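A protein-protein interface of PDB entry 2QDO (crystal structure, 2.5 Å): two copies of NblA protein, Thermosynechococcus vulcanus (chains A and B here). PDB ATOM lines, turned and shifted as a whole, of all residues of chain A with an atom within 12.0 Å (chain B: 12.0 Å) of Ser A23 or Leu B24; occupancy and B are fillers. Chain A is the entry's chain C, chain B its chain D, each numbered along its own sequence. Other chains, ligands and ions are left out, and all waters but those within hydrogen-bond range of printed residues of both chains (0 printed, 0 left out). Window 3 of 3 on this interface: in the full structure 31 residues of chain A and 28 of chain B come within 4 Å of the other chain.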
ATOM      1  N   MET A  15     -31.836  22.881   2.503  1.00  0.00           N
ATOM      2  CA  MET A  15     -31.030  21.663   2.506  1.00  0.00           C
ATOM      3  C   MET A  15     -31.203  20.988   3.861  1.00  0.00           C
ATOM      4  O   MET A  15     -31.273  19.761   3.952  1.00  0.00           O
ATOM      5  CB  MET A  15     -29.549  21.985   2.279  1.00  0.00           C
ATOM      6  CG  MET A  15     -28.635  20.766   2.145  1.00  0.00           C
ATOM      7  SD  MET A  15     -28.778  19.933   0.545  1.00  0.00           S
ATOM      8  CE  MET A  15     -28.392  21.316  -0.568  1.00  0.00           C
ATOM      9  N   GLU A  16     -31.274  21.797   4.914  1.00  0.00           N
ATOM     10  CA  GLU A  16     -31.451  21.273   6.262  1.00  0.00           C
ATOM     11  C   GLU A  16     -32.800  20.583   6.406  1.00  0.00           C
ATOM     12  O   GLU A  16     -32.954  19.690   7.239  1.00  0.00           O
ATOM     13  CB  GLU A  16     -31.350  22.384   7.312  1.00  0.00           C
ATOM     14  CG  GLU A  16     -31.545  21.885   8.750  1.00  0.00           C
ATOM     15  CD  GLU A  16     -31.778  23.007   9.749  1.00  0.00           C
ATOM     16  OE1 GLU A  16     -32.445  23.992   9.370  1.00  0.00           O
ATOM     17  OE2 GLU A  16     -31.320  22.907  10.913  1.00  0.00           O
ATOM     18  N   GLU A  17     -33.780  21.000   5.610  1.00  0.00           N
ATOM     19  CA  GLU A  17     -35.089  20.370   5.682  1.00  0.00           C
ATOM     20  C   GLU A  17     -34.963  18.967   5.105  1.00  0.00           C
ATOM     21  O   GLU A  17     -35.359  17.979   5.726  1.00  0.00           O
ATOM     22  CB  GLU A  17     -36.133  21.162   4.879  1.00  0.00           C
ATOM     23  CG  GLU A  17     -36.664  22.480   5.493  1.00  0.00           C
ATOM     24  CD  GLU A  17     -36.094  22.848   6.859  1.00  0.00           C
ATOM     25  OE1 GLU A  17     -34.972  22.428   7.198  1.00  0.00           O
ATOM     26  OE2 GLU A  17     -36.771  23.597   7.595  1.00  0.00           O
ATOM     27  N   GLN A  18     -34.369  18.901   3.921  1.00  0.00           N
ATOM     28  CA  GLN A  18     -34.197  17.660   3.186  1.00  0.00           C
ATOM     29  C   GLN A  18     -33.148  16.698   3.736  1.00  0.00           C
ATOM     30  O   GLN A  18     -33.196  15.506   3.450  1.00  0.00           O
ATOM     31  CB  GLN A  18     -33.888  17.991   1.726  1.00  0.00           C
ATOM     32  CG  GLN A  18     -34.797  19.079   1.180  1.00  0.00           C
ATOM     33  CD  GLN A  18     -34.474  19.468  -0.243  1.00  0.00           C
ATOM     34  OE1 GLN A  18     -33.331  19.366  -0.678  1.00  0.00           O
ATOM     35  NE2 GLN A  18     -35.480  19.940  -0.972  1.00  0.00           N
ATOM     36  N   VAL A  19     -32.198  17.202   4.515  1.00  0.00           N
ATOM     37  CA  VAL A  19     -31.166  16.339   5.074  1.00  0.00           C
ATOM     38  C   VAL A  19     -31.694  15.576   6.295  1.00  0.00           C
ATOM     39  O   VAL A  19     -31.398  14.388   6.472  1.00  0.00           O
ATOM     40  CB  VAL A  19     -29.884  17.178   5.422  1.00  0.00           C
ATOM     41  CG1 VAL A  19     -29.002  16.452   6.432  1.00  0.00           C
ATOM     42  CG2 VAL A  19     -29.072  17.415   4.145  1.00  0.00           C
ATOM     43  N   SER A  20     -32.506  16.253   7.105  1.00  0.00           N
ATOM     44  CA  SER A  20     -33.090  15.681   8.321  1.00  0.00           C
ATOM     45  C   SER A  20     -33.961  14.446   8.084  1.00  0.00           C
ATOM     46  O   SER A  20     -34.194  13.654   8.999  1.00  0.00           O
ATOM     47  CB  SER A  20     -33.939  16.732   9.025  1.00  0.00           C
ATOM     48  OG  SER A  20     -35.130  16.967   8.294  1.00  0.00           O
ATOM     49  N   ALA A  21     -34.451  14.299   6.861  1.00  0.00           N
ATOM     50  CA  ALA A  21     -35.293  13.173   6.508  1.00  0.00           C
ATOM     51  C   ALA A  21     -34.544  12.233   5.567  1.00  0.00           C
ATOM     52  O   ALA A  21     -35.152  11.455   4.837  1.00  0.00           O
ATOM     53  CB  ALA A  21     -36.567  13.682   5.849  1.00  0.00           C
ATOM     54  N   MET A  22     -33.219  12.310   5.585  1.00  0.00           N
ATOM     55  CA  MET A  22     -32.392  11.458   4.730  1.00  0.00           C
ATOM     56  C   MET A  22     -31.966  10.163   5.410  1.00  0.00           C
ATOM     57  O   MET A  22     -31.692  10.140   6.613  1.00  0.00           O
ATOM     58  CB  MET A  22     -31.142  12.212   4.274  1.00  0.00           C
ATOM     59  CG  MET A  22     -31.346  13.085   3.054  1.00  0.00           C
ATOM     60  SD  MET A  22     -29.846  13.992   2.641  1.00  0.00           S
ATOM     61  CE  MET A  22     -29.045  12.844   1.594  1.00  0.00           C
ATOM     62  N   SER A  23     -31.912   9.087   4.628  1.00  0.00           N
ATOM     63  CA  SER A  23     -31.504   7.783   5.141  1.00  0.00           C
ATOM     64  C   SER A  23     -29.984   7.774   5.264  1.00  0.00           C
ATOM     65  O   SER A  23     -29.314   8.658   4.726  1.00  0.00           O
ATOM     66  CB  SER A  23     -31.948   6.682   4.184  1.00  0.00           C
ATOM     67  OG  SER A  23     -31.152   6.672   3.013  1.00  0.00           O
ATOM     68  N   LEU A  24     -29.434   6.784   5.963  1.00  0.00           N
ATOM     69  CA  LEU A  24     -27.984   6.713   6.122  1.00  0.00           C
ATOM     70  C   LEU A  24     -27.279   6.552   4.776  1.00  0.00           C
ATOM     71  O   LEU A  24     -26.204   7.118   4.564  1.00  0.00           O
ATOM     72  CB  LEU A  24     -27.588   5.566   7.058  1.00  0.00           C
ATOM     73  CG  LEU A  24     -26.089   5.481   7.372  1.00  0.00           C
ATOM     74  CD1 LEU A  24     -25.586   6.837   7.836  1.00  0.00           C
ATOM     75  CD2 LEU A  24     -25.841   4.428   8.439  1.00  0.00           C
ATOM     76  N   GLN A  25     -27.893   5.792   3.870  1.00  0.00           N
ATOM     77  CA  GLN A  25     -27.321   5.567   2.546  1.00  0.00           C
ATOM     78  C   GLN A  25     -27.345   6.869   1.727  1.00  0.00           C
ATOM     79  O   GLN A  25     -26.309   7.294   1.213  1.00  0.00           O
ATOM     80  CB  GLN A  25     -28.080   4.431   1.814  1.00  0.00           C
ATOM     81  CG  GLN A  25     -27.289   3.745   0.674  1.00  0.00           C
ATOM     82  CD  GLN A  25     -28.005   2.542   0.039  1.00  0.00           C
ATOM     83  OE1 GLN A  25     -28.133   1.478   0.649  1.00  0.00           O
ATOM     84  NE2 GLN A  25     -28.466   2.715  -1.197  1.00  0.00           N
ATOM     85  N   GLU A  26     -28.507   7.519   1.625  1.00  0.00           N
ATOM     86  CA  GLU A  26     -28.605   8.763   0.852  1.00  0.00           C
ATOM     87  C   GLU A  26     -27.664   9.869   1.347  1.00  0.00           C
ATOM     88  O   GLU A  26     -27.046  10.561   0.541  1.00  0.00           O
ATOM     89  CB  GLU A  26     -30.043   9.311   0.830  1.00  0.00           C
ATOM     90  CG  GLU A  26     -30.261  10.255  -0.363  1.00  0.00           C
ATOM     91  CD  GLU A  26     -31.603  10.966  -0.383  1.00  0.00           C
ATOM     92  OE1 GLU A  26     -32.444  10.713   0.505  1.00  0.00           O
ATOM     93  OE2 GLU A  26     -31.811  11.788  -1.304  1.00  0.00           O
ATOM     94  N   ALA A  27     -27.560  10.035   2.662  1.00  0.00           N
ATOM     95  CA  ALA A  27     -26.700  11.057   3.236  1.00  0.00           C
ATOM     96  C   ALA A  27     -25.232  10.775   2.937  1.00  0.00           C
ATOM     97  O   ALA A  27     -24.422  11.698   2.836  1.00  0.00           O
ATOM     98  CB  ALA A  27     -26.917  11.141   4.741  1.00  0.00           C
ATOM     99  N   ARG A  28     -24.891   9.498   2.794  1.00  0.00           N
ATOM    100  CA  ARG A  28     -23.518   9.120   2.513  1.00  0.00           C
ATOM    101  C   ARG A  28     -23.185   9.273   1.034  1.00  0.00           C
ATOM    102  O   ARG A  28     -22.115   9.779   0.701  1.00  0.00           O
ATOM    103  CB  ARG A  28     -23.251   7.689   2.980  1.00  0.00           C
ATOM    104  CG  ARG A  28     -23.042   7.558   4.480  1.00  0.00           C
ATOM    105  CD  ARG A  28     -22.771   6.110   4.860  1.00  0.00           C
ATOM    106  NE  ARG A  28     -22.401   5.940   6.264  1.00  0.00           N
ATOM    107  CZ  ARG A  28     -22.398   4.765   6.887  1.00  0.00           C
ATOM    108  NH1 ARG A  28     -22.049   4.683   8.161  1.00  0.00           N
ATOM    109  NH2 ARG A  28     -22.749   3.664   6.234  1.00  0.00           N
ATOM    110  N   GLU A  29     -24.077   8.849   0.138  1.00  0.00           N
ATOM    111  CA  GLU A  29     -23.775   9.009  -1.284  1.00  0.00           C
ATOM    112  C   GLU A  29     -23.643  10.499  -1.602  1.00  0.00           C
ATOM    113  O   GLU A  29     -22.652  10.913  -2.217  1.00  0.00           O
ATOM    114  CB  GLU A  29     -24.848   8.385  -2.191  1.00  0.00           C
ATOM    115  CG  GLU A  29     -24.870   8.932  -3.659  1.00  0.00           C
ATOM    116  CD  GLU A  29     -23.596   8.677  -4.491  1.00  0.00           C
ATOM    117  OE1 GLU A  29     -23.704   8.112  -5.603  1.00  0.00           O
ATOM    118  OE2 GLU A  29     -22.491   9.061  -4.058  1.00  0.00           O
ATOM    119  N   LEU A  30     -24.619  11.294  -1.153  1.00  0.00           N
ATOM    120  CA  LEU A  30     -24.615  12.741  -1.398  1.00  0.00           C
ATOM    121  C   LEU A  30     -23.395  13.456  -0.810  1.00  0.00           C
ATOM    122  O   LEU A  30     -22.814  14.302  -1.478  1.00  0.00           O
ATOM    123  CB  LEU A  30     -25.906  13.392  -0.864  1.00  0.00           C
ATOM    124  CG  LEU A  30     -27.238  13.025  -1.535  1.00  0.00           C
ATOM    125  CD1 LEU A  30     -28.286  14.032  -1.130  1.00  0.00           C
ATOM    126  CD2 LEU A  30     -27.105  13.033  -3.071  1.00  0.00           C
ATOM    127  N   LEU A  31     -23.010  13.119   0.423  1.00  0.00           N
ATOM    128  CA  LEU A  31     -21.853  13.736   1.085  1.00  0.00           C
ATOM    129  C   LEU A  31     -20.606  13.485   0.238  1.00  0.00           C
ATOM    130  O   LEU A  31     -19.740  14.353   0.092  1.00  0.00           O
ATOM    131  CB  LEU A  31     -21.631  13.111   2.464  1.00  0.00           C
ATOM    132  CG  LEU A  31     -21.018  13.889   3.638  1.00  0.00           C
ATOM    133  CD1 LEU A  31     -20.371  12.874   4.583  1.00  0.00           C
ATOM    134  CD2 LEU A  31     -19.969  14.911   3.170  1.00  0.00           C
ATOM    135  N   LEU A  32     -20.512  12.271  -0.294  1.00  0.00           N
ATOM    136  CA  LEU A  32     -19.386  11.885  -1.128  1.00  0.00           C
ATOM    137  C   LEU A  32     -19.443  12.663  -2.423  1.00  0.00           C
ATOM    138  O   LEU A  32     -18.411  13.065  -2.957  1.00  0.00           O
ATOM    139  CB  LEU A  32     -19.433  10.385  -1.419  1.00  0.00           C
ATOM    140  CG  LEU A  32     -18.314   9.542  -0.811  1.00  0.00           C
ATOM    141  CD1 LEU A  32     -17.988  10.058   0.563  1.00  0.00           C
ATOM    142  CD2 LEU A  32     -18.744   8.086  -0.750  1.00  0.00           C
ATOM    143  N   GLN B  18     -14.066   7.176   5.319  1.00  0.00           N
ATOM    144  CA  GLN B  18     -14.591   7.839   6.517  1.00  0.00           C
ATOM    145  C   GLN B  18     -16.115   7.840   6.520  1.00  0.00           C
ATOM    146  O   GLN B  18     -16.753   7.536   7.530  1.00  0.00           O
ATOM    147  CB  GLN B  18     -14.103   9.286   6.597  1.00  0.00           C
ATOM    148  CG  GLN B  18     -12.692   9.461   7.117  1.00  0.00           C
ATOM    149  CD  GLN B  18     -12.156  10.845   6.835  1.00  0.00           C
ATOM    150  OE1 GLN B  18     -12.083  11.268   5.682  1.00  0.00           O
ATOM    151  NE2 GLN B  18     -11.775  11.560   7.885  1.00  0.00           N
ATOM    152  N   VAL B  19     -16.687   8.205   5.382  1.00  0.00           N
ATOM    153  CA  VAL B  19     -18.124   8.247   5.231  1.00  0.00           C
ATOM    154  C   VAL B  19     -18.707   6.891   5.588  1.00  0.00           C
ATOM    155  O   VAL B  19     -19.598   6.789   6.433  1.00  0.00           O
ATOM    156  CB  VAL B  19     -18.497   8.617   3.784  1.00  0.00           C
ATOM    157  CG1 VAL B  19     -19.964   8.339   3.526  1.00  0.00           C
ATOM    158  CG2 VAL B  19     -18.189  10.084   3.549  1.00  0.00           C
ATOM    159  N   SER B  20     -18.177   5.850   4.948  1.00  0.00           N
ATOM    160  CA  SER B  20     -18.625   4.479   5.157  1.00  0.00           C
ATOM    161  C   SER B  20     -18.634   4.068   6.628  1.00  0.00           C
ATOM    162  O   SER B  20     -19.156   3.013   6.971  1.00  0.00           O
ATOM    163  CB  SER B  20     -17.723   3.512   4.402  1.00  0.00           C
ATOM    164  OG  SER B  20     -16.563   3.238   5.173  1.00  0.00           O
ATOM    165  N   ALA B  21     -18.034   4.880   7.493  1.00  0.00           N
ATOM    166  CA  ALA B  21     -17.990   4.566   8.923  1.00  0.00           C
ATOM    167  C   ALA B  21     -18.785   5.579   9.721  1.00  0.00           C
ATOM    168  O   ALA B  21     -18.937   5.455  10.935  1.00  0.00           O
ATOM    169  CB  ALA B  21     -16.561   4.567   9.409  1.00  0.00           C
ATOM    170  N   MET B  22     -19.296   6.584   9.024  1.00  0.00           N
ATOM    171  CA  MET B  22     -20.042   7.666   9.644  1.00  0.00           C
ATOM    172  C   MET B  22     -21.417   7.316  10.180  1.00  0.00           C
ATOM    173  O   MET B  22     -22.097   6.438   9.667  1.00  0.00           O
ATOM    174  CB  MET B  22     -20.174   8.805   8.640  1.00  0.00           C
ATOM    175  CG  MET B  22     -19.682  10.149   9.119  1.00  0.00           C
ATOM    176  SD  MET B  22     -19.278  11.174   7.702  1.00  0.00           S
ATOM    177  CE  MET B  22     -17.475  11.121   7.788  1.00  0.00           C
ATOM    178  N   SER B  23     -21.816   8.001  11.241  1.00  0.00           N
ATOM    179  CA  SER B  23     -23.138   7.775  11.799  1.00  0.00           C
ATOM    180  C   SER B  23     -24.095   8.619  10.957  1.00  0.00           C
ATOM    181  O   SER B  23     -23.672   9.565  10.287  1.00  0.00           O
ATOM    182  CB  SER B  23     -23.188   8.226  13.261  1.00  0.00           C
ATOM    183  OG  SER B  23     -23.236   9.640  13.364  1.00  0.00           O
ATOM    184  N   LEU B  24     -25.376   8.276  10.976  1.00  0.00           N
ATOM    185  CA  LEU B  24     -26.372   9.037  10.227  1.00  0.00           C
ATOM    186  C   LEU B  24     -26.341  10.501  10.705  1.00  0.00           C
ATOM    187  O   LEU B  24     -26.641  11.421   9.947  1.00  0.00           O
ATOM    188  CB  LEU B  24     -27.770   8.457  10.465  1.00  0.00           C
ATOM    189  CG  LEU B  24     -28.916   9.346   9.977  1.00  0.00           C
ATOM    190  CD1 LEU B  24     -28.769   9.571   8.477  1.00  0.00           C
ATOM    191  CD2 LEU B  24     -30.259   8.699  10.298  1.00  0.00           C
ATOM    192  N   GLN B  25     -25.979  10.688  11.975  1.00  0.00           N
ATOM    193  CA  GLN B  25     -25.902  12.006  12.607  1.00  0.00           C
ATOM    194  C   GLN B  25     -24.788  12.870  12.020  1.00  0.00           C
ATOM    195  O   GLN B  25     -25.030  13.985  11.559  1.00  0.00           O
ATOM    196  CB  GLN B  25     -25.691  11.836  14.116  1.00  0.00           C
ATOM    197  CG  GLN B  25     -25.629  13.119  14.949  1.00  0.00           C
ATOM    198  CD  GLN B  25     -26.207  14.343  14.258  1.00  0.00           C
ATOM    199  OE1 GLN B  25     -27.117  14.243  13.441  1.00  0.00           O
ATOM    200  NE2 GLN B  25     -25.686  15.515  14.604  1.00  0.00           N
ATOM    201  N   GLU B  26     -23.568  12.350  12.029  1.00  0.00           N
ATOM    202  CA  GLU B  26     -22.441  13.094  11.493  1.00  0.00           C
ATOM    203  C   GLU B  26     -22.586  13.251   9.976  1.00  0.00           C
ATOM    204  O   GLU B  26     -22.337  14.327   9.432  1.00  0.00           O
ATOM    205  CB  GLU B  26     -21.129  12.387  11.846  1.00  0.00           C
ATOM    206  CG  GLU B  26     -19.911  13.290  11.776  1.00  0.00           C
ATOM    207  CD  GLU B  26     -18.612  12.566  12.065  1.00  0.00           C
ATOM    208  OE1 GLU B  26     -18.512  11.361  11.754  1.00  0.00           O
ATOM    209  OE2 GLU B  26     -17.679  13.212  12.582  1.00  0.00           O
ATOM    210  N   ALA B  27     -23.011  12.186   9.301  1.00  0.00           N
ATOM    211  CA  ALA B  27     -23.189  12.242   7.859  1.00  0.00           C
ATOM    212  C   ALA B  27     -24.098  13.405   7.469  1.00  0.00           C
ATOM    213  O   ALA B  27     -23.938  13.973   6.390  1.00  0.00           O
ATOM    214  CB  ALA B  27     -23.766  10.937   7.342  1.00  0.00           C
ATOM    215  N   ARG B  28     -25.047  13.758   8.335  1.00  0.00           N
ATOM    216  CA  ARG B  28     -25.946  14.876   8.047  1.00  0.00           C
ATOM    217  C   ARG B  28     -25.295  16.231   8.350  1.00  0.00           C
ATOM    218  O   ARG B  28     -25.308  17.131   7.504  1.00  0.00           O
ATOM    219  CB  ARG B  28     -27.231  14.749   8.854  1.00  0.00           C
ATOM    220  CG  ARG B  28     -28.242  13.788   8.281  1.00  0.00           C
ATOM    221  CD  ARG B  28     -29.280  13.468   9.332  1.00  0.00           C
ATOM    222  NE  ARG B  28     -30.420  12.731   8.806  1.00  0.00           N
ATOM    223  CZ  ARG B  28     -31.348  12.170   9.571  1.00  0.00           C
ATOM    224  NH1 ARG B  28     -32.359  11.519   9.020  1.00  0.00           N
ATOM    225  NH2 ARG B  28     -31.255  12.249  10.894  1.00  0.00           N
ATOM    226  N   GLU B  29     -24.733  16.371   9.549  1.00  0.00           N
ATOM    227  CA  GLU B  29     -24.090  17.618   9.946  1.00  0.00           C
ATOM    228  C   GLU B  29     -23.121  18.020   8.841  1.00  0.00           C
ATOM    229  O   GLU B  29     -23.198  19.123   8.305  1.00  0.00           O
ATOM    230  CB  GLU B  29     -23.344  17.436  11.279  1.00  0.00           C
ATOM    231  N   LEU B  30     -22.237  17.090   8.493  1.00  0.00           N
ATOM    232  CA  LEU B  30     -21.231  17.282   7.462  1.00  0.00           C
ATOM    233  C   LEU B  30     -21.758  17.501   6.043  1.00  0.00           C
ATOM    234  O   LEU B  30     -21.094  18.155   5.236  1.00  0.00           O
ATOM    235  CB  LEU B  30     -20.271  16.097   7.478  1.00  0.00           C
ATOM    236  CG  LEU B  30     -18.870  16.301   8.067  1.00  0.00           C
ATOM    237  CD1 LEU B  30     -18.900  17.188   9.307  1.00  0.00           C
ATOM    238  CD2 LEU B  30     -18.284  14.929   8.388  1.00  0.00           C
ATOM    239  N   LEU B  31     -22.928  16.962   5.723  1.00  0.00           N
ATOM    240  CA  LEU B  31     -23.492  17.148   4.381  1.00  0.00           C
ATOM    241  C   LEU B  31     -23.892  18.615   4.285  1.00  0.00           C
ATOM    242  O   LEU B  31     -23.826  19.217   3.214  1.00  0.00           O
ATOM    243  CB  LEU B  31     -24.755  16.305   4.176  1.00  0.00           C
ATOM    244  CG  LEU B  31     -25.137  15.717   2.810  1.00  0.00           C
ATOM    245  CD1 LEU B  31     -26.657  15.539   2.801  1.00  0.00           C
ATOM    246  CD2 LEU B  31     -24.724  16.611   1.651  1.00  0.00           C
ATOM    247  N   LEU B  32     -24.342  19.168   5.411  1.00  0.00           N
ATOM    248  CA  LEU B  32     -24.760  20.567   5.463  1.00  0.00           C
ATOM    249  C   LEU B  32     -23.566  21.456   5.326  1.00  0.00           C
ATOM    250  O   LEU B  32     -23.552  22.351   4.485  1.00  0.00           O
ATOM    251  CB  LEU B  32     -25.468  20.899   6.774  1.00  0.00           C
ATOM    252  CG  LEU B  32     -26.923  20.453   6.797  1.00  0.00           C
ATOM    253  CD1 LEU B  32     -27.683  21.186   7.891  1.00  0.00           C
ATOM    254  CD2 LEU B  32     -27.534  20.729   5.434  1.00  0.00           C
ATOM    255  N   GLN B  33     -22.565  21.201   6.159  1.00  0.00           N
ATOM    256  CA  GLN B  33     -21.358  21.988   6.108  1.00  0.00           C
ATOM    257  C   GLN B  33     -20.815  22.044   4.691  1.00  0.00           C
ATOM    258  O   GLN B  33     -20.458  23.116   4.215  1.00  0.00           O
ATOM    259  CB  GLN B  33     -20.295  21.419   7.037  1.00  0.00           C
ATOM    260  CG  GLN B  33     -18.972  22.128   6.877  1.00  0.00           C
ATOM    261  CD  GLN B  33     -17.972  21.743   7.927  1.00  0.00           C
ATOM    262  OE1 GLN B  33     -18.260  21.815   9.118  1.00  0.00           O
ATOM    263  NE2 GLN B  33     -16.778  21.342   7.497  1.00  0.00           N
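NE of Arg B28 lies within hydrogen-bond range of O of Val A19 (3.0 Å).
O of Ser A20 is in hydrogen-bond range of NH1 of Arg B28.
The guanidinium group (NH1) of Arg B28 is in hydrogen-bond range of the backbone carbonyl oxygen (O) of Met A22 (2.9 Å).
The guanidinium group of Arg A28 sits at hydrogen-bond distance from the backbone carbonyl oxygen of Val B19.
NE of Arg A28 lies close to O of Met B22, 3.5 Å away.
The backbone carbonyl oxygen of Glu A17 lies within hydrogen-bond range of the side-chain hydroxyl of Ser A20.
The side-chain hydroxyl (OG) of Ser A23 lies close to the backbone NH (N) of Gln A25.
N of Glu A26 sits at hydrogen-bond distance from OG of Ser A23 (3.1 Å).
The side-chain hydroxyl (OG) of Ser B23 sits close to the backbone NH (N) of Gln B25 (3.2 Å).
The side-chain hydroxyl (OG) of Ser B23 lies within hydrogen-bond range of the backbone NH (N) of Glu B26 (3.0 Å).
Among the printed residues, pairs that only touch across the chains: Leu A32 with Val B19, Val A19 with Leu B31, Leu A24 with Leu B24, Met A15 with Leu B32, Met A22 with Leu B24, Arg A28 with Ser B20, Met A22 with Leu B31, Leu A31 with Val B19, Leu A31 with Met B22, Arg A28 with Ala B21, Val A19 with Leu B32, Ser A23 with Leu B24, Leu A24 with Ser B23, Glu A16 with Leu B32 and Leu A24 with Met B22.
Printed residues of chain B within 4 Å of Ser A23: Leu B24 (3.9 Å).
Leu B24 touches just these residues of chain A: Met A22, Ser A23 and Leu A24.
No residue of chain B comes within 4 Å of Gln A25.
No residue of chain B comes within 4 Å of Glu A26.
No residue of chain B comes within 4 Å of Ala A27.
No residue of chain A comes within 4 Å of Gln B25.
Of the printed residues of chain A, Arg B28 touches Val A19, Ser A20 and Met A22.
Printed residues of chain A within 4 Å of Leu B31: Val A19 (3.3 Å) and Met A22 (3.5 Å).
Printed residues of chain A within 4 Å of Val B19: Arg A28, Leu A31 and Leu A32.
Of the printed residues of chain A, Leu B32 touches Met A15, Glu A16 and Val A19.
Printed residues of chain B within 4 Å of Arg A28: Val B19, Ser B20, Ala B21 and Met B22.
Printed residues of chain B within 4 Å of Leu A31: Val B19 and Met B22.
Gln B18 touches none of the printed residues of chain A.
The nearest residue of chain B that does not touch Ser A23 is Arg B28 (5.0 Å).
The nearest residue of chain A that does not touch Leu B24 is Ala A27 (4.5 Å).
The nearest printed residue of chain A that does not touch Val B19 is Glu A29 (5.4 Å).
Among the printed residues, 20 pairs touch across the chains.
Among the printed residues, no Asp or Glu carboxylate lies within 4 Å of a Lys or Arg side-chain nitrogen of the other chain.
Val A19 touches Leu B31, and with the chains exchanged Leu A31 touches Val B19.
Val A19 touches Leu B32, and with the chains exchanged Leu A32 touches Val B19.
Ser A20 touches Arg B28, and with the chains exchanged Arg A28 touches Ser B20.
Met A22 touches Leu B24, and with the chains exchanged Leu A24 touches Met B22.
Of the 20 pairs that touch across the chains among the printed residues, 17 have their exchanged pair printed and touching as well.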
